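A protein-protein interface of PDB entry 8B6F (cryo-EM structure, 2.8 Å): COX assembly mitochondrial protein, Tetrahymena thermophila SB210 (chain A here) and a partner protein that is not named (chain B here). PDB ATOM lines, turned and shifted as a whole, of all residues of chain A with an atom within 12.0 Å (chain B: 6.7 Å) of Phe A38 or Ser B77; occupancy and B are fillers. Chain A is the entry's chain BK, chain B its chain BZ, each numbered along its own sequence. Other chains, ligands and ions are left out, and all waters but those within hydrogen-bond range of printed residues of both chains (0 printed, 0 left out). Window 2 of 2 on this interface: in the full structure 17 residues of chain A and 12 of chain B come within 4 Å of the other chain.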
ATOM      1  N   MET A  36      18.564 -20.846 -10.949  1.00  0.00           N
ATOM      2  CA  MET A  36      18.131 -22.009 -10.126  1.00  0.00           C
ATOM      3  C   MET A  36      17.151 -22.874 -10.905  1.00  0.00           C
ATOM      4  O   MET A  36      16.779 -23.958 -10.459  1.00  0.00           O
ATOM      5  CB  MET A  36      17.501 -21.539  -8.814  1.00  0.00           C
ATOM      6  CG  MET A  36      16.293 -20.639  -8.989  1.00  0.00           C
ATOM      7  SD  MET A  36      15.725 -19.913  -7.440  1.00  0.00           S
ATOM      8  CE  MET A  36      15.397 -21.380  -6.466  1.00  0.00           C
ATOM      9  N   GLU A  37      16.726 -22.383 -12.070  1.00  0.00           N
ATOM     10  CA  GLU A  37      15.846 -23.176 -12.921  1.00  0.00           C
ATOM     11  C   GLU A  37      16.543 -24.434 -13.420  1.00  0.00           C
ATOM     12  O   GLU A  37      15.880 -25.435 -13.708  1.00  0.00           O
ATOM     13  CB  GLU A  37      15.355 -22.338 -14.103  1.00  0.00           C
ATOM     14  CG  GLU A  37      16.454 -21.807 -15.022  1.00  0.00           C
ATOM     15  CD  GLU A  37      17.053 -20.501 -14.541  1.00  0.00           C
ATOM     16  OE1 GLU A  37      16.830 -20.140 -13.368  1.00  0.00           O
ATOM     17  OE2 GLU A  37      17.744 -19.833 -15.336  1.00  0.00           O
ATOM     18  N   PHE A  38      17.869 -24.401 -13.531  1.00  0.00           N
ATOM     19  CA  PHE A  38      18.646 -25.545 -13.993  1.00  0.00           C
ATOM     20  C   PHE A  38      19.139 -26.427 -12.856  1.00  0.00           C
ATOM     21  O   PHE A  38      19.802 -27.434 -13.119  1.00  0.00           O
ATOM     22  CB  PHE A  38      19.853 -25.063 -14.805  1.00  0.00           C
ATOM     23  CG  PHE A  38      19.500 -24.135 -15.928  1.00  0.00           C
ATOM     24  CD1 PHE A  38      18.392 -24.373 -16.721  1.00  0.00           C
ATOM     25  CD2 PHE A  38      20.276 -23.019 -16.184  1.00  0.00           C
ATOM     26  CE1 PHE A  38      18.067 -23.519 -17.753  1.00  0.00           C
ATOM     27  CE2 PHE A  38      19.956 -22.159 -17.214  1.00  0.00           C
ATOM     28  CZ  PHE A  38      18.849 -22.410 -18.001  1.00  0.00           C
ATOM     29  N   SER A  39      18.833 -26.079 -11.610  1.00  0.00           N
ATOM     30  CA  SER A  39      19.388 -26.765 -10.450  1.00  0.00           C
ATOM     31  C   SER A  39      18.491 -27.940 -10.079  1.00  0.00           C
ATOM     32  O   SER A  39      17.361 -27.748  -9.621  1.00  0.00           O
ATOM     33  CB  SER A  39      19.538 -25.796  -9.281  1.00  0.00           C
ATOM     34  OG  SER A  39      20.065 -26.461  -8.149  1.00  0.00           O
ATOM     35  N   ASN A  40      18.996 -29.158 -10.281  1.00  0.00           N
ATOM     36  CA  ASN A  40      18.229 -30.346  -9.918  1.00  0.00           C
ATOM     37  C   ASN A  40      17.961 -30.394  -8.421  1.00  0.00           C
ATOM     38  O   ASN A  40      16.863 -30.765  -7.990  1.00  0.00           O
ATOM     39  CB  ASN A  40      18.967 -31.607 -10.366  1.00  0.00           C
ATOM     40  CG  ASN A  40      19.065 -31.720 -11.872  1.00  0.00           C
ATOM     41  OD1 ASN A  40      20.159 -31.748 -12.433  1.00  0.00           O
ATOM     42  ND2 ASN A  40      17.918 -31.788 -12.535  1.00  0.00           N
ATOM     43  N   ALA A  41      18.955 -30.033  -7.608  1.00  0.00           N
ATOM     44  CA  ALA A  41      18.771 -30.056  -6.162  1.00  0.00           C
ATOM     45  C   ALA A  41      17.682 -29.082  -5.729  1.00  0.00           C
ATOM     46  O   ALA A  41      16.794 -29.436  -4.946  1.00  0.00           O
ATOM     47  CB  ALA A  41      20.090 -29.730  -5.464  1.00  0.00           C
ATOM     48  N   LEU A  42      17.727 -27.850  -6.235  1.00  0.00           N
ATOM     49  CA  LEU A  42      16.726 -26.861  -5.848  1.00  0.00           C
ATOM     50  C   LEU A  42      15.342 -27.244  -6.354  1.00  0.00           C
ATOM     51  O   LEU A  42      14.338 -26.986  -5.681  1.00  0.00           O
ATOM     52  CB  LEU A  42      17.132 -25.480  -6.360  1.00  0.00           C
ATOM     53  CG  LEU A  42      18.446 -24.935  -5.797  1.00  0.00           C
ATOM     54  CD1 LEU A  42      18.836 -23.643  -6.487  1.00  0.00           C
ATOM     55  CD2 LEU A  42      18.341 -24.709  -4.301  1.00  0.00           C
ATOM     56  N   LEU A  43      15.263 -27.856  -7.535  1.00  0.00           N
ATOM     57  CA  LEU A  43      13.971 -28.303  -8.042  1.00  0.00           C
ATOM     58  C   LEU A  43      13.432 -29.483  -7.245  1.00  0.00           C
ATOM     59  O   LEU A  43      12.214 -29.608  -7.075  1.00  0.00           O
ATOM     60  CB  LEU A  43      14.079 -28.663  -9.523  1.00  0.00           C
ATOM     61  CG  LEU A  43      14.272 -27.481 -10.477  1.00  0.00           C
ATOM     62  CD1 LEU A  43      14.578 -27.970 -11.877  1.00  0.00           C
ATOM     63  CD2 LEU A  43      13.044 -26.583 -10.489  1.00  0.00           C
ATOM     64  N   SER A  44      14.310 -30.360  -6.757  1.00  0.00           N
ATOM     65  CA  SER A  44      13.850 -31.471  -5.933  1.00  0.00           C
ATOM     66  C   SER A  44      13.440 -31.002  -4.544  1.00  0.00           C
ATOM     67  O   SER A  44      12.605 -31.642  -3.895  1.00  0.00           O
ATOM     68  CB  SER A  44      14.936 -32.542  -5.834  1.00  0.00           C
ATOM     69  OG  SER A  44      16.104 -32.031  -5.215  1.00  0.00           O
ATOM     70  N   GLN A  45      14.023 -29.901  -4.064  1.00  0.00           N
ATOM     71  CA  GLN A  45      13.602 -29.330  -2.793  1.00  0.00           C
ATOM     72  C   GLN A  45      12.178 -28.792  -2.844  1.00  0.00           C
ATOM     73  O   GLN A  45      11.561 -28.608  -1.791  1.00  0.00           O
ATOM     74  CB  GLN A  45      14.567 -28.223  -2.376  1.00  0.00           C
ATOM     75  CG  GLN A  45      15.928 -28.741  -1.944  1.00  0.00           C
ATOM     76  CD  GLN A  45      16.929 -27.629  -1.719  1.00  0.00           C
ATOM     77  OE1 GLN A  45      16.564 -26.459  -1.627  1.00  0.00           O
ATOM     78  NE2 GLN A  45      18.205 -27.990  -1.634  1.00  0.00           N
ATOM     79  N   THR A  46      11.645 -28.536  -4.036  1.00  0.00           N
ATOM     80  CA  THR A  46      10.261 -28.108  -4.162  1.00  0.00           C
ATOM     81  C   THR A  46       9.319 -29.275  -3.882  1.00  0.00           C
ATOM     82  O   THR A  46       9.683 -30.447  -4.003  1.00  0.00           O
ATOM     83  CB  THR A  46       9.991 -27.544  -5.558  1.00  0.00           C
ATOM     84  OG1 THR A  46      10.302 -28.533  -6.547  1.00  0.00           O
ATOM     85  CG2 THR A  46      10.825 -26.298  -5.806  1.00  0.00           C
ATOM     86  N   ARG A  99      16.438 -39.455  -8.254  1.00  0.00           N
ATOM     87  CA  ARG A  99      17.401 -38.794  -9.129  1.00  0.00           C
ATOM     88  C   ARG A  99      18.707 -38.532  -8.393  1.00  0.00           C
ATOM     89  O   ARG A  99      19.795 -38.801  -8.915  1.00  0.00           O
ATOM     90  CB  ARG A  99      16.815 -37.487  -9.659  1.00  0.00           C
ATOM     91  CG  ARG A  99      17.612 -36.875 -10.797  1.00  0.00           C
ATOM     92  CD  ARG A  99      17.305 -37.575 -12.110  1.00  0.00           C
ATOM     93  NE  ARG A  99      18.389 -37.438 -13.076  1.00  0.00           N
ATOM     94  CZ  ARG A  99      19.376 -38.309 -13.233  1.00  0.00           C
ATOM     95  NH1 ARG A  99      19.450 -39.411 -12.505  1.00  0.00           N
ATOM     96  NH2 ARG A  99      20.313 -38.069 -14.145  1.00  0.00           N
ATOM     97  N   ASP A 103      22.393 -40.231  -9.330  1.00  0.00           N
ATOM     98  CA  ASP A 103      23.563 -39.407  -9.611  1.00  0.00           C
ATOM     99  C   ASP A 103      24.699 -39.731  -8.651  1.00  0.00           C
ATOM    100  O   ASP A 103      25.860 -39.835  -9.061  1.00  0.00           O
ATOM    101  CB  ASP A 103      23.196 -37.926  -9.523  1.00  0.00           C
ATOM    102  CG  ASP A 103      22.175 -37.518 -10.564  1.00  0.00           C
ATOM    103  OD1 ASP A 103      22.168 -38.123 -11.657  1.00  0.00           O
ATOM    104  OD2 ASP A 103      21.383 -36.593 -10.292  1.00  0.00           O
ATOM    105  N   TYR B  69      26.114 -29.803 -12.243  1.00  0.00           N
ATOM    106  CA  TYR B  69      25.187 -28.714 -12.530  1.00  0.00           C
ATOM    107  C   TYR B  69      25.602 -27.952 -13.781  1.00  0.00           C
ATOM    108  O   TYR B  69      24.758 -27.605 -14.615  1.00  0.00           O
ATOM    109  CB  TYR B  69      25.106 -27.766 -11.335  1.00  0.00           C
ATOM    110  CG  TYR B  69      24.336 -26.500 -11.622  1.00  0.00           C
ATOM    111  CD1 TYR B  69      22.954 -26.464 -11.504  1.00  0.00           C
ATOM    112  CD2 TYR B  69      24.991 -25.338 -12.004  1.00  0.00           C
ATOM    113  CE1 TYR B  69      22.246 -25.308 -11.764  1.00  0.00           C
ATOM    114  CE2 TYR B  69      24.292 -24.177 -12.266  1.00  0.00           C
ATOM    115  CZ  TYR B  69      22.920 -24.169 -12.145  1.00  0.00           C
ATOM    116  OH  TYR B  69      22.219 -23.016 -12.406  1.00  0.00           O
ATOM    117  N   ARG B  72      24.718 -29.929 -17.019  1.00  0.00           N
ATOM    118  CA  ARG B  72      23.286 -29.929 -17.291  1.00  0.00           C
ATOM    119  C   ARG B  72      22.754 -28.519 -17.499  1.00  0.00           C
ATOM    120  O   ARG B  72      21.824 -28.320 -18.287  1.00  0.00           O
ATOM    121  CB  ARG B  72      22.538 -30.621 -16.155  1.00  0.00           C
ATOM    122  CG  ARG B  72      22.955 -32.064 -15.956  1.00  0.00           C
ATOM    123  CD  ARG B  72      22.188 -32.719 -14.825  1.00  0.00           C
ATOM    124  NE  ARG B  72      22.598 -34.104 -14.633  1.00  0.00           N
ATOM    125  CZ  ARG B  72      22.095 -34.916 -13.715  1.00  0.00           C
ATOM    126  NH1 ARG B  72      21.154 -34.514 -12.876  1.00  0.00           N
ATOM    127  NH2 ARG B  72      22.544 -36.164 -13.636  1.00  0.00           N
ATOM    128  N   ALA B  73      23.321 -27.533 -16.805  1.00  0.00           N
ATOM    129  CA  ALA B  73      22.924 -26.150 -17.040  1.00  0.00           C
ATOM    130  C   ALA B  73      23.285 -25.709 -18.453  1.00  0.00           C
ATOM    131  O   ALA B  73      22.523 -24.983 -19.100  1.00  0.00           O
ATOM    132  CB  ALA B  73      23.579 -25.234 -16.009  1.00  0.00           C
ATOM    133  N   LYS B  74      24.450 -26.136 -18.945  1.00  0.00           N
ATOM    134  CA  LYS B  74      24.856 -25.782 -20.301  1.00  0.00           C
ATOM    135  C   LYS B  74      23.888 -26.345 -21.332  1.00  0.00           C
ATOM    136  O   LYS B  74      23.510 -25.651 -22.282  1.00  0.00           O
ATOM    137  CB  LYS B  74      26.273 -26.293 -20.562  1.00  0.00           C
ATOM    138  CG  LYS B  74      26.835 -25.950 -21.934  1.00  0.00           C
ATOM    139  CD  LYS B  74      27.070 -24.459 -22.085  1.00  0.00           C
ATOM    140  CE  LYS B  74      27.769 -24.144 -23.398  1.00  0.00           C
ATOM    141  NZ  LYS B  74      28.091 -22.697 -23.522  1.00  0.00           N
ATOM    142  N   LEU B  75      23.477 -27.602 -21.162  1.00  0.00           N
ATOM    143  CA  LEU B  75      22.563 -28.216 -22.121  1.00  0.00           C
ATOM    144  C   LEU B  75      21.211 -27.518 -22.122  1.00  0.00           C
ATOM    145  O   LEU B  75      20.603 -27.328 -23.181  1.00  0.00           O
ATOM    146  CB  LEU B  75      22.400 -29.704 -21.811  1.00  0.00           C
ATOM    147  CG  LEU B  75      23.654 -30.568 -21.963  1.00  0.00           C
ATOM    148  CD1 LEU B  75      23.369 -31.997 -21.547  1.00  0.00           C
ATOM    149  CD2 LEU B  75      24.179 -30.533 -23.386  1.00  0.00           C
ATOM    150  N   GLN B  76      20.718 -27.135 -20.944  1.00  0.00           N
ATOM    151  CA  GLN B  76      19.444 -26.432 -20.864  1.00  0.00           C
ATOM    152  C   GLN B  76      19.548 -24.987 -21.328  1.00  0.00           C
ATOM    153  O   GLN B  76      18.529 -24.395 -21.700  1.00  0.00           O
ATOM    154  CB  GLN B  76      18.912 -26.481 -19.434  1.00  0.00           C
ATOM    155  CG  GLN B  76      18.638 -27.884 -18.936  1.00  0.00           C
ATOM    156  CD  GLN B  76      18.144 -27.902 -17.510  1.00  0.00           C
ATOM    157  OE1 GLN B  76      16.944 -27.826 -17.257  1.00  0.00           O
ATOM    158  NE2 GLN B  76      19.069 -28.003 -16.564  1.00  0.00           N
ATOM    159  N   SER B  77      20.748 -24.406 -21.320  1.00  0.00           N
ATOM    160  CA  SER B  77      20.942 -23.048 -21.810  1.00  0.00           C
ATOM    161  C   SER B  77      21.019 -22.971 -23.329  1.00  0.00           C
ATOM    162  O   SER B  77      21.009 -21.864 -23.876  1.00  0.00           O
ATOM    163  CB  SER B  77      22.219 -22.452 -21.213  1.00  0.00           C
ATOM    164  OG  SER B  77      22.163 -22.435 -19.798  1.00  0.00           O
ATOM    165  N   LEU B  78      21.098 -24.109 -24.013  1.00  0.00           N
ATOM    166  CA  LEU B  78      21.193 -24.104 -25.465  1.00  0.00           C
ATOM    167  C   LEU B  78      20.005 -23.375 -26.076  1.00  0.00           C
ATOM    168  O   LEU B  78      18.860 -23.550 -25.653  1.00  0.00           O
ATOM    169  CB  LEU B  78      21.254 -25.537 -25.995  1.00  0.00           C
ATOM    170  CG  LEU B  78      22.439 -26.379 -25.520  1.00  0.00           C
ATOM    171  CD1 LEU B  78      22.288 -27.813 -25.990  1.00  0.00           C
ATOM    172  CD2 LEU B  78      23.749 -25.792 -26.007  1.00  0.00           C
ATOM    173  N   LYS B  79      20.286 -22.550 -27.079  1.00  0.00           N
ATOM    174  CA  LYS B  79      19.230 -21.830 -27.768  1.00  0.00           C
ATOM    175  C   LYS B  79      18.339 -22.804 -28.530  1.00  0.00           C
ATOM    176  O   LYS B  79      18.739 -23.916 -28.878  1.00  0.00           O
ATOM    177  CB  LYS B  79      19.819 -20.792 -28.724  1.00  0.00           C
ATOM    178  CG  LYS B  79      20.208 -19.478 -28.057  1.00  0.00           C
ATOM    179  CD  LYS B  79      21.307 -19.664 -27.023  1.00  0.00           C
ATOM    180  CE  LYS B  79      21.703 -18.332 -26.404  1.00  0.00           C
ATOM    181  NZ  LYS B  79      22.775 -18.489 -25.382  1.00  0.00           N
ATOM    182  N   ILE B  80      17.102 -22.368 -28.780  1.00  0.00           N
ATOM    183  CA  ILE B  80      16.138 -23.217 -29.468  1.00  0.00           C
ATOM    184  C   ILE B  80      16.720 -23.667 -30.799  1.00  0.00           C
ATOM    185  O   ILE B  80      17.222 -22.855 -31.586  1.00  0.00           O
ATOM    186  CB  ILE B  80      14.809 -22.468 -29.649  1.00  0.00           C
ATOM    187  CG1 ILE B  80      13.737 -23.391 -30.236  1.00  0.00           C
ATOM    188  CG2 ILE B  80      14.991 -21.242 -30.536  1.00  0.00           C
ATOM    189  CD1 ILE B  80      13.329 -24.522 -29.323  1.00  0.00           C
ATOM    190  N   GLU B  82      19.321 -25.773 -31.156  1.00  0.00           N
ATOM    191  CA  GLU B  82      20.679 -26.271 -30.998  1.00  0.00           C
ATOM    192  C   GLU B  82      20.755 -27.594 -30.251  1.00  0.00           C
ATOM    193  O   GLU B  82      21.805 -28.242 -30.283  1.00  0.00           O
ATOM    194  CB  GLU B  82      21.522 -25.242 -30.244  1.00  0.00           C
ATOM    195  CG  GLU B  82      21.629 -23.906 -30.943  1.00  0.00           C
ATOM    196  CD  GLU B  82      22.562 -22.955 -30.227  1.00  0.00           C
ATOM    197  OE1 GLU B  82      23.234 -23.389 -29.270  1.00  0.00           O
ATOM    198  OE2 GLU B  82      22.628 -21.775 -30.624  1.00  0.00           O
ATOM    199  N   GLU B  83      19.677 -28.015 -29.590  1.00  0.00           N
ATOM    200  CA  GLU B  83      19.730 -29.247 -28.813  1.00  0.00           C
ATOM    201  C   GLU B  83      19.741 -30.488 -29.694  1.00  0.00           C
ATOM    202  O   GLU B  83      20.154 -31.554 -29.229  1.00  0.00           O
ATOM    203  CB  GLU B  83      18.559 -29.317 -27.827  1.00  0.00           C
ATOM    204  CG  GLU B  83      17.215 -28.887 -28.389  1.00  0.00           C
ATOM    205  CD  GLU B  83      16.949 -27.402 -28.211  1.00  0.00           C
ATOM    206  OE1 GLU B  83      17.861 -26.684 -27.753  1.00  0.00           O
ATOM    207  OE2 GLU B  83      15.830 -26.950 -28.529  1.00  0.00           O
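The side-chain amide oxygen (OD1) of Asn A40 lies within hydrogen-bond range of the guanidinium group (NH1) of Arg B72, 3.0 Å away. OD1 of Asp A103 is in salt-bridge range of NH2 of Arg B72 (2.8 Å). The guanidinium group (NH2) of Arg B72 lies close to the guanidinium group (NH2) of Arg A99 (3.0 Å).
N of Leu A42 lies close to OG of Ser A39 (3.3 Å). The backbone carbonyl oxygen (O) of Asn A40 sits at hydrogen-bond distance from the side-chain hydroxyl (OG) of Ser A44. NH2 of Arg A99 is in salt-bridge range of OD1 of Asp A103. The backbone carbonyl oxygen of Arg B72 lies within hydrogen-bond range of the side-chain amide nitrogen of Gln B76. The backbone carbonyl oxygen (O) of Ala B73 sits at hydrogen-bond distance from the side-chain hydroxyl (OG) of Ser B77, 2.7 Å away.
Hydrophobic or aromatic side chains of chain A within 4 Å of the printed part of chain B: Phe A38. Of the 12 printed residues of chain B, 5 touch a printed residue of chain A. Printed residues of chain B that touch a printed residue of chain A: Tyr B69, Arg B72, Ala B73, Gln B76 and Ser B77. Hydrophobic or aromatic side chains of chain B within 4 Å of the printed part of chain A: Tyr B69 and Ala B73. Along chain B the printed residues that touch a printed residue of chain A span positions 69 to 77. Among the printed residues, Asp or Glu carboxylates within 4 Å of a Lys or Arg side-chain nitrogen of the other chain: Asp A103 with Arg B72.
Among the printed residues, pairs that only touch across the chains: Phe A38 with Ser B77 (3.4 Å), Ser A39 with Tyr B69 (3.5 Å), Phe A38 with Gln B76 (3.5 Å), Phe A38 with Tyr B69 (3.5 Å) and Phe A38 with Ala B73 (3.9 Å).
Ser B77 touches just one residue of chain A: Phe A38. Of chain A, only Phe A38 and Ser A39 come within 4 Å of Tyr B69. Ala B73 touches just one residue of chain A: Phe A38 (3.9 Å). No residue of chain A comes within 4 Å of Lys B74. Gln B76 touches just one residue of chain A: Phe A38 (3.5 Å). No residue of chain A comes within 4 Å of Leu B78. No residue of chain A comes within 4 Å of Lys B79. Printed residues of chain B within 4 Å of Arg A99: Arg B72. Of the printed residues of chain B, Asn A40 touches Arg B72 (3.0 Å). Of the printed residues of chain B, Ser A39 touches Tyr B69 (3.5 Å). Of the printed residues of chain A, Arg B72 touches Asn A40, Arg A99 and Asp A103. Of the printed residues of chain B, Asp A103 touches Arg B72. Ser A44 touches none of the printed residues of chain B. The nearest residue of chain A that does not touch Ser B77 is Glu A37 (6.8 Å). The nearest printed residue of chain A that does not touch Arg B72 is Phe A38 (5.2 Å).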
